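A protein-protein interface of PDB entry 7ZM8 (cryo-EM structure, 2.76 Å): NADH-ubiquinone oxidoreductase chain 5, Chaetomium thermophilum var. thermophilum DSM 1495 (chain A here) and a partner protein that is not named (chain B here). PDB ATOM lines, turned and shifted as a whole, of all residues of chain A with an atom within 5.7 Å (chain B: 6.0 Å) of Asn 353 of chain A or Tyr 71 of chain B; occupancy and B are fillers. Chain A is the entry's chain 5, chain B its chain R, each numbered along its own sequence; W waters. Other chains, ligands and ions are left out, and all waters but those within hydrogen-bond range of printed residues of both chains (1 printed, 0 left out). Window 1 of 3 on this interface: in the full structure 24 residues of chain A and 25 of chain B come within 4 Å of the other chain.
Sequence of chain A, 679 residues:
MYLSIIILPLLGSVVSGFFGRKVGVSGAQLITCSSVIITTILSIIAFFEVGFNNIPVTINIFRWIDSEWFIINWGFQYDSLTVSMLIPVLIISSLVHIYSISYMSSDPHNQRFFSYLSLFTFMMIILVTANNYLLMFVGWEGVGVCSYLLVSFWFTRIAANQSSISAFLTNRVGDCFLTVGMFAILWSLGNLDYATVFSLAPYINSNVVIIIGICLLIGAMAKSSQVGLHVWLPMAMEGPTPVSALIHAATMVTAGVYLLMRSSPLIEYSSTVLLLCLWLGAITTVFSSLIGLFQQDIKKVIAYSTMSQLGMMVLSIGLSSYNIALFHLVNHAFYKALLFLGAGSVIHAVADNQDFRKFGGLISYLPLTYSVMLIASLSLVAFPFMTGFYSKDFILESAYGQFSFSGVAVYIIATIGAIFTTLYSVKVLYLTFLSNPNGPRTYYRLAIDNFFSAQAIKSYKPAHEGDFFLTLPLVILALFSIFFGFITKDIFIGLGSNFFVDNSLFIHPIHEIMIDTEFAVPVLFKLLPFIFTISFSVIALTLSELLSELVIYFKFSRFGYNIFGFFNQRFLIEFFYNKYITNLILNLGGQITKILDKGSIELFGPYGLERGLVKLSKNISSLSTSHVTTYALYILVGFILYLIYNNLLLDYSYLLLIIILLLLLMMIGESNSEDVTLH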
ATOM      1  N   VAL A 346     -11.631 -18.222 -18.782  1.00  0.00           N
ATOM      2  CA  VAL A 346     -10.556 -19.039 -19.334  1.00  0.00           C
ATOM      3  C   VAL A 346     -10.566 -20.424 -18.706  1.00  0.00           C
ATOM      4  O   VAL A 346     -10.156 -21.399 -19.343  1.00  0.00           O
ATOM      5  CB  VAL A 346      -9.184 -18.355 -19.170  1.00  0.00           C
ATOM      6  CG1 VAL A 346      -9.238 -16.942 -19.657  1.00  0.00           C
ATOM      7  CG2 VAL A 346      -8.680 -18.422 -17.748  1.00  0.00           C
ATOM      8  N   ILE A 347     -11.026 -20.546 -17.460  1.00  0.00           N
ATOM      9  CA  ILE A 347     -11.214 -21.869 -16.872  1.00  0.00           C
ATOM     10  C   ILE A 347     -12.275 -22.637 -17.645  1.00  0.00           C
ATOM     11  O   ILE A 347     -12.163 -23.848 -17.853  1.00  0.00           O
ATOM     12  CB  ILE A 347     -11.586 -21.755 -15.382  1.00  0.00           C
ATOM     13  CG1 ILE A 347     -10.591 -20.881 -14.630  1.00  0.00           C
ATOM     14  CG2 ILE A 347     -11.638 -23.121 -14.742  1.00  0.00           C
ATOM     15  CD1 ILE A 347     -11.090 -20.461 -13.270  1.00  0.00           C
ATOM     16  N   VAL A 350     -10.724 -23.799 -21.046  1.00  0.00           N
ATOM     17  CA  VAL A 350      -9.635 -24.823 -20.993  1.00  0.00           C
ATOM     18  C   VAL A 350     -10.031 -26.035 -20.152  1.00  0.00           C
ATOM     19  O   VAL A 350      -9.171 -26.524 -19.390  1.00  0.00           O
ATOM     20  CB  VAL A 350      -8.269 -24.240 -20.586  1.00  0.00           C
ATOM     21  CG1 VAL A 350      -7.778 -23.207 -21.586  1.00  0.00           C
ATOM     22  CG2 VAL A 350      -8.268 -23.673 -19.178  1.00  0.00           C
ATOM     23  N   ALA A 351     -11.265 -26.522 -20.300  1.00  0.00           N
ATOM     24  CA  ALA A 351     -11.648 -27.784 -19.631  1.00  0.00           C
ATOM     25  C   ALA A 351     -11.461 -27.734 -18.117  1.00  0.00           C
ATOM     26  O   ALA A 351     -10.942 -28.723 -17.568  1.00  0.00           O
ATOM     27  CB  ALA A 351     -10.862 -28.918 -20.225  1.00  0.00           C
ATOM     28  N   ASP A 352     -11.837 -26.632 -17.476  1.00  0.00           N
ATOM     29  CA  ASP A 352     -11.799 -26.556 -15.997  1.00  0.00           C
ATOM     30  C   ASP A 352     -10.394 -26.782 -15.468  1.00  0.00           C
ATOM     31  O   ASP A 352     -10.272 -27.283 -14.372  1.00  0.00           O
ATOM     32  CB  ASP A 352     -12.853 -27.443 -15.335  1.00  0.00           C
ATOM     33  CG  ASP A 352     -14.166 -26.735 -15.048  1.00  0.00           C
ATOM     34  OD1 ASP A 352     -14.197 -25.494 -15.140  1.00  0.00           O
ATOM     35  OD2 ASP A 352     -15.147 -27.432 -14.735  1.00  0.00           O
ATOM     36  N   ASN A 353      -9.358 -26.415 -16.223  1.00  0.00           N
ATOM     37  CA  ASN A 353      -7.988 -26.473 -15.647  1.00  0.00           C
ATOM     38  C   ASN A 353      -7.731 -25.105 -15.013  1.00  0.00           C
ATOM     39  O   ASN A 353      -8.095 -24.097 -15.641  1.00  0.00           O
ATOM     40  CB  ASN A 353      -6.927 -26.832 -16.689  1.00  0.00           C
ATOM     41  CG  ASN A 353      -5.537 -26.968 -16.102  1.00  0.00           C
ATOM     42  OD1 ASN A 353      -5.264 -27.891 -15.340  1.00  0.00           O
ATOM     43  ND2 ASN A 353      -4.650 -26.054 -16.455  1.00  0.00           N
ATOM     44  N   GLN A 354      -7.174 -25.073 -13.803  1.00  0.00           N
ATOM     45  CA  GLN A 354      -6.970 -23.786 -13.094  1.00  0.00           C
ATOM     46  C   GLN A 354      -5.476 -23.544 -12.887  1.00  0.00           C
ATOM     47  O   GLN A 354      -5.144 -22.639 -12.119  1.00  0.00           O
ATOM     48  CB  GLN A 354      -7.711 -23.812 -11.758  1.00  0.00           C
ATOM     49  CG  GLN A 354      -9.224 -23.774 -11.882  1.00  0.00           C
ATOM     50  CD  GLN A 354      -9.881 -23.782 -10.524  1.00  0.00           C
ATOM     51  OE1 GLN A 354      -9.225 -23.935  -9.498  1.00  0.00           O
ATOM     52  NE2 GLN A 354     -11.192 -23.618 -10.510  1.00  0.00           N
ATOM     53  N   ASP A 355      -4.612 -24.299 -13.567  1.00  0.00           N
ATOM     54  CA  ASP A 355      -3.147 -24.186 -13.325  1.00  0.00           C
ATOM     55  C   ASP A 355      -2.474 -23.401 -14.454  1.00  0.00           C
ATOM     56  O   ASP A 355      -2.683 -23.764 -15.621  1.00  0.00           O
ATOM     57  CB  ASP A 355      -2.519 -25.566 -13.104  1.00  0.00           C
ATOM     58  CG  ASP A 355      -1.231 -25.558 -12.301  1.00  0.00           C
ATOM     59  OD1 ASP A 355      -0.429 -24.623 -12.479  1.00  0.00           O
ATOM     60  OD2 ASP A 355      -1.044 -26.489 -11.500  1.00  0.00           O
ATOM     61  N   PHE A 356      -1.665 -22.395 -14.103  1.00  0.00           N
ATOM     62  CA  PHE A 356      -0.930 -21.574 -15.100  1.00  0.00           C
ATOM     63  C   PHE A 356       0.036 -22.459 -15.883  1.00  0.00           C
ATOM     64  O   PHE A 356       0.265 -22.174 -17.070  1.00  0.00           O
ATOM     65  CB  PHE A 356      -0.048 -20.533 -14.409  1.00  0.00           C
ATOM     66  CG  PHE A 356      -0.755 -19.465 -13.618  1.00  0.00           C
ATOM     67  CD1 PHE A 356      -1.502 -18.489 -14.252  1.00  0.00           C
ATOM     68  CD2 PHE A 356      -0.630 -19.408 -12.241  1.00  0.00           C
ATOM     69  CE1 PHE A 356      -2.138 -17.499 -13.523  1.00  0.00           C
ATOM     70  CE2 PHE A 356      -1.265 -18.418 -11.512  1.00  0.00           C
ATOM     71  CZ  PHE A 356      -2.017 -17.463 -12.155  1.00  0.00           C
ATOM     72  N   ARG A 357       0.589 -23.487 -15.238  1.00  0.00           N
ATOM     73  CA  ARG A 357       1.617 -24.350 -15.878  1.00  0.00           C
ATOM     74  C   ARG A 357       1.040 -25.110 -17.075  1.00  0.00           C
ATOM     75  O   ARG A 357       1.840 -25.667 -17.845  1.00  0.00           O
ATOM     76  CB  ARG A 357       2.199 -25.311 -14.837  1.00  0.00           C
ATOM     77  CG  ARG A 357       2.863 -24.614 -13.660  1.00  0.00           C
ATOM     78  CD  ARG A 357       3.328 -25.569 -12.579  1.00  0.00           C
ATOM     79  NE  ARG A 357       2.252 -25.886 -11.656  1.00  0.00           N
ATOM     80  CZ  ARG A 357       2.396 -26.614 -10.557  1.00  0.00           C
ATOM     81  NH1 ARG A 357       3.582 -27.104 -10.239  1.00  0.00           N
ATOM     82  NH2 ARG A 357       1.357 -26.841  -9.777  1.00  0.00           N
ATOM     83  N   LYS A 358      -0.287 -25.157 -17.206  1.00  0.00           N
ATOM     84  CA  LYS A 358      -0.929 -25.850 -18.356  1.00  0.00           C
ATOM     85  C   LYS A 358      -1.685 -24.862 -19.248  1.00  0.00           C
ATOM     86  O   LYS A 358      -2.535 -25.320 -20.027  1.00  0.00           O
ATOM     87  CB  LYS A 358      -1.798 -27.016 -17.876  1.00  0.00           C
ATOM     88  CG  LYS A 358      -1.057 -28.066 -17.066  1.00  0.00           C
ATOM     89  CD  LYS A 358      -0.023 -28.831 -17.860  1.00  0.00           C
ATOM     90  CE  LYS A 358       1.012 -29.498 -16.979  1.00  0.00           C
ATOM     91  NZ  LYS A 358       1.860 -30.444 -17.742  1.00  0.00           N
ATOM     92  N   PHE A 359      -1.413 -23.563 -19.121  1.00  0.00           N
ATOM     93  CA  PHE A 359      -2.043 -22.557 -20.019  1.00  0.00           C
ATOM     94  C   PHE A 359      -0.949 -21.916 -20.867  1.00  0.00           C
ATOM     95  O   PHE A 359       0.155 -21.717 -20.340  1.00  0.00           O
ATOM     96  CB  PHE A 359      -2.666 -21.388 -19.252  1.00  0.00           C
ATOM     97  CG  PHE A 359      -3.712 -21.710 -18.216  1.00  0.00           C
ATOM     98  CD1 PHE A 359      -4.555 -22.799 -18.353  1.00  0.00           C
ATOM     99  CD2 PHE A 359      -3.877 -20.885 -17.117  1.00  0.00           C
ATOM    100  CE1 PHE A 359      -5.512 -23.069 -17.390  1.00  0.00           C
ATOM    101  CE2 PHE A 359      -4.842 -21.149 -16.161  1.00  0.00           C
ATOM    102  CZ  PHE A 359      -5.660 -22.242 -16.302  1.00  0.00           C
ATOM    103  N   TYR A 443      -6.664 -27.947 -26.631  1.00  0.00           N
ATOM    104  CA  TYR A 443      -7.096 -26.556 -26.560  1.00  0.00           C
ATOM    105  C   TYR A 443      -6.669 -25.754 -27.775  1.00  0.00           C
ATOM    106  O   TYR A 443      -7.178 -24.649 -27.978  1.00  0.00           O
ATOM    107  CB  TYR A 443      -6.555 -25.830 -25.323  1.00  0.00           C
ATOM    108  CG  TYR A 443      -6.538 -26.591 -24.028  1.00  0.00           C
ATOM    109  CD1 TYR A 443      -7.658 -27.277 -23.585  1.00  0.00           C
ATOM    110  CD2 TYR A 443      -5.404 -26.612 -23.242  1.00  0.00           C
ATOM    111  CE1 TYR A 443      -7.644 -27.966 -22.394  1.00  0.00           C
ATOM    112  CE2 TYR A 443      -5.384 -27.282 -22.047  1.00  0.00           C
ATOM    113  CZ  TYR A 443      -6.502 -27.966 -21.629  1.00  0.00           C
ATOM    114  OH  TYR A 443      -6.475 -28.650 -20.437  1.00  0.00           O
ATOM    115  N   LYS B  16       8.362 -35.685 -13.740  1.00  0.00           N
ATOM    116  CA  LYS B  16       7.277 -34.796 -13.339  1.00  0.00           C
ATOM    117  C   LYS B  16       7.786 -33.683 -12.433  1.00  0.00           C
ATOM    118  O   LYS B  16       7.337 -32.537 -12.537  1.00  0.00           O
ATOM    119  CB  LYS B  16       6.174 -35.585 -12.643  1.00  0.00           C
ATOM    120  CG  LYS B  16       5.352 -36.445 -13.568  1.00  0.00           C
ATOM    121  CD  LYS B  16       3.951 -36.652 -13.018  1.00  0.00           C
ATOM    122  CE  LYS B  16       2.924 -36.711 -14.137  1.00  0.00           C
ATOM    123  NZ  LYS B  16       2.798 -35.406 -14.840  1.00  0.00           N
ATOM    124  N   ASP B  20       7.608 -29.569 -13.020  1.00  0.00           N
ATOM    125  CA  ASP B  20       6.829 -28.847 -11.991  1.00  0.00           C
ATOM    126  C   ASP B  20       7.624 -27.611 -11.605  1.00  0.00           C
ATOM    127  O   ASP B  20       7.029 -26.536 -11.510  1.00  0.00           O
ATOM    128  CB  ASP B  20       6.394 -29.768 -10.859  1.00  0.00           C
ATOM    129  CG  ASP B  20       5.120 -30.529 -11.160  1.00  0.00           C
ATOM    130  OD1 ASP B  20       4.481 -30.218 -12.184  1.00  0.00           O
ATOM    131  OD2 ASP B  20       4.780 -31.427 -10.371  1.00  0.00           O
ATOM    132  N   ASP B  69       3.773 -27.517  -4.484  1.00  0.00           N
ATOM    133  CA  ASP B  69       2.462 -27.712  -5.101  1.00  0.00           C
ATOM    134  C   ASP B  69       2.652 -28.414  -6.433  1.00  0.00           C
ATOM    135  O   ASP B  69       2.736 -27.776  -7.488  1.00  0.00           O
ATOM    136  CB  ASP B  69       1.741 -26.376  -5.286  1.00  0.00           C
ATOM    137  CG  ASP B  69       0.248 -26.483  -5.049  1.00  0.00           C
ATOM    138  OD1 ASP B  69      -0.261 -27.619  -4.932  1.00  0.00           O
ATOM    139  OD2 ASP B  69      -0.418 -25.430  -4.977  1.00  0.00           O
ATOM    140  N   PRO B  70       2.742 -29.739  -6.423  1.00  0.00           N
ATOM    141  CA  PRO B  70       2.887 -30.466  -7.682  1.00  0.00           C
ATOM    142  C   PRO B  70       1.629 -30.340  -8.521  1.00  0.00           C
ATOM    143  O   PRO B  70       0.516 -30.212  -8.007  1.00  0.00           O
ATOM    144  CB  PRO B  70       3.114 -31.915  -7.235  1.00  0.00           C
ATOM    145  CG  PRO B  70       3.361 -31.848  -5.767  1.00  0.00           C
ATOM    146  CD  PRO B  70       2.631 -30.653  -5.282  1.00  0.00           C
ATOM    147  N   TYR B  71       1.817 -30.367  -9.832  1.00  0.00           N
ATOM    148  CA  TYR B  71       0.680 -30.280 -10.730  1.00  0.00           C
ATOM    149  C   TYR B  71      -0.188 -31.527 -10.624  1.00  0.00           C
ATOM    150  O   TYR B  71       0.311 -32.647 -10.518  1.00  0.00           O
ATOM    151  CB  TYR B  71       1.152 -30.099 -12.168  1.00  0.00           C
ATOM    152  CG  TYR B  71       0.072 -30.384 -13.175  1.00  0.00           C
ATOM    153  CD1 TYR B  71      -0.972 -29.493 -13.367  1.00  0.00           C
ATOM    154  CD2 TYR B  71       0.086 -31.543 -13.926  1.00  0.00           C
ATOM    155  CE1 TYR B  71      -1.968 -29.748 -14.280  1.00  0.00           C
ATOM    156  CE2 TYR B  71      -0.902 -31.804 -14.840  1.00  0.00           C
ATOM    157  CZ  TYR B  71      -1.927 -30.903 -15.016  1.00  0.00           C
ATOM    158  OH  TYR B  71      -2.915 -31.164 -15.930  1.00  0.00           O
ATOM    159  N   CYS B  72      -1.507 -31.350 -10.623  1.00  0.00           N
ATOM    160  CA  CYS B  72      -2.465 -32.487 -10.642  1.00  0.00           C
ATOM    161  C   CYS B  72      -3.446 -32.222 -11.783  1.00  0.00           C
ATOM    162  O   CYS B  72      -3.909 -31.079 -11.896  1.00  0.00           O
ATOM    163  CB  CYS B  72      -3.240 -32.589  -9.335  1.00  0.00           C
ATOM    164  SG  CYS B  72      -3.886 -34.252  -9.043  1.00  0.00           S
ATOM    165  N   PRO B  73      -3.740 -33.197 -12.665  1.00  0.00           N
ATOM    166  CA  PRO B  73      -4.741 -32.991 -13.708  1.00  0.00           C
ATOM    167  C   PRO B  73      -6.066 -32.662 -13.007  1.00  0.00           C
ATOM    168  O   PRO B  73      -6.304 -33.182 -11.949  1.00  0.00           O
ATOM    169  CB  PRO B  73      -4.748 -34.341 -14.433  1.00  0.00           C
ATOM    170  CG  PRO B  73      -3.388 -34.925 -14.160  1.00  0.00           C
ATOM    171  CD  PRO B  73      -3.073 -34.494 -12.746  1.00  0.00           C
ATOM    172  N   PRO B  74      -6.953 -31.823 -13.577  1.00  0.00           N
ATOM    173  CA  PRO B  74      -8.163 -31.359 -12.857  1.00  0.00           C
ATOM    174  C   PRO B  74      -9.136 -32.417 -12.331  1.00  0.00           C
ATOM    175  O   PRO B  74      -9.692 -32.195 -11.302  1.00  0.00           O
ATOM    176  CB  PRO B  74      -8.878 -30.498 -13.899  1.00  0.00           C
ATOM    177  CG  PRO B  74      -7.789 -30.068 -14.846  1.00  0.00           C
ATOM    178  CD  PRO B  74      -6.837 -31.241 -14.910  1.00  0.00           C
HETATM  179  O   HOH W   1      -2.388 -28.860 -10.335  1.00  0.00           O
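Asn 353 of chain A touches two residues of chain B. Printed residues of chain B within 4 Å of Lys 358 of chain A: Tyr 71. Of the printed residues of chain A, Asp 20 of chain B touches Arg 357. Of the printed residues of chain A, Pro 70 of chain B touches Arg 357. Of chain A, only Asn 353 (3.9 Å), Asp 355 (3.5 Å), Arg 357 (3.6 Å) and Lys 358 (3.4 Å) come within 4 Å of Tyr 71 of chain B. Of the printed residues of chain A, Pro 74 of chain B touches Asp 352 (3.5 Å) and Asn 353 (3.4 Å). The nearest printed residue of chain A that does not touch Pro 74 of chain B is Ala 351 of chain A (4.4 Å).
Of the 13 printed residues of chain A, 5 touch a printed residue of chain B. Of the 8 printed residues of chain B, 5 touch a printed residue of chain A. Hydrophobic or aromatic side chains of chain B within 4 Å of the printed part of chain A: Tyr 71 and Pro 74. Among the printed residues, Asp or Glu carboxylates within 4 Å of a Lys or Arg side-chain nitrogen of the other chain: Arg 357 of chain A with Asp 20 of chain B (3.8 Å).
Among the printed residues, pairs that only touch across the chains: Asn 353 of chain A with Pro 74 of chain B, Lys 358 of chain A with Tyr 71 of chain B, Asp 352 of chain A with Pro 74 of chain B, Asp 355 of chain A with Tyr 71 of chain B, Arg 357 of chain A with Tyr 71 of chain B, Arg 357 of chain A with Pro 70 of chain B and Asn 353 of chain A with Tyr 71 of chain B.
Water W1 lies within hydrogen-bond range of the backbone NH of Cys 72 of chain B (2.7 Å) and the side-chain carboxylate of Asp 355 of chain A (3.0 Å).
The side-chain carboxylate of Asp 20 of chain B lies within salt-bridge range of the guanidinium group of Arg 357 of chain A (3.8 Å). The backbone carbonyl oxygen (O) of Asp 69 of chain B lies within hydrogen-bond range of the guanidinium group (NH2) of Arg 357 of chain A (2.8 Å).
The guanidinium group (NH2) of Arg 357 of chain A is in salt-bridge range of the side-chain carboxylate (OD2) of Asp 355 of chain A (3.0 Å). N of Tyr 71 of chain B lies within hydrogen-bond range of OD2 of Asp 20 of chain B, at 3.2 Å. The backbone carbonyl oxygen of Asp 355 of chain A is in hydrogen-bond range of the side-chain amide nitrogen of Asn 353 of chain A (3.1 Å). The backbone carbonyl oxygen (O) of Ile 347 of chain A sits at hydrogen-bond distance from the backbone NH (N) of Asp 352 of chain A.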
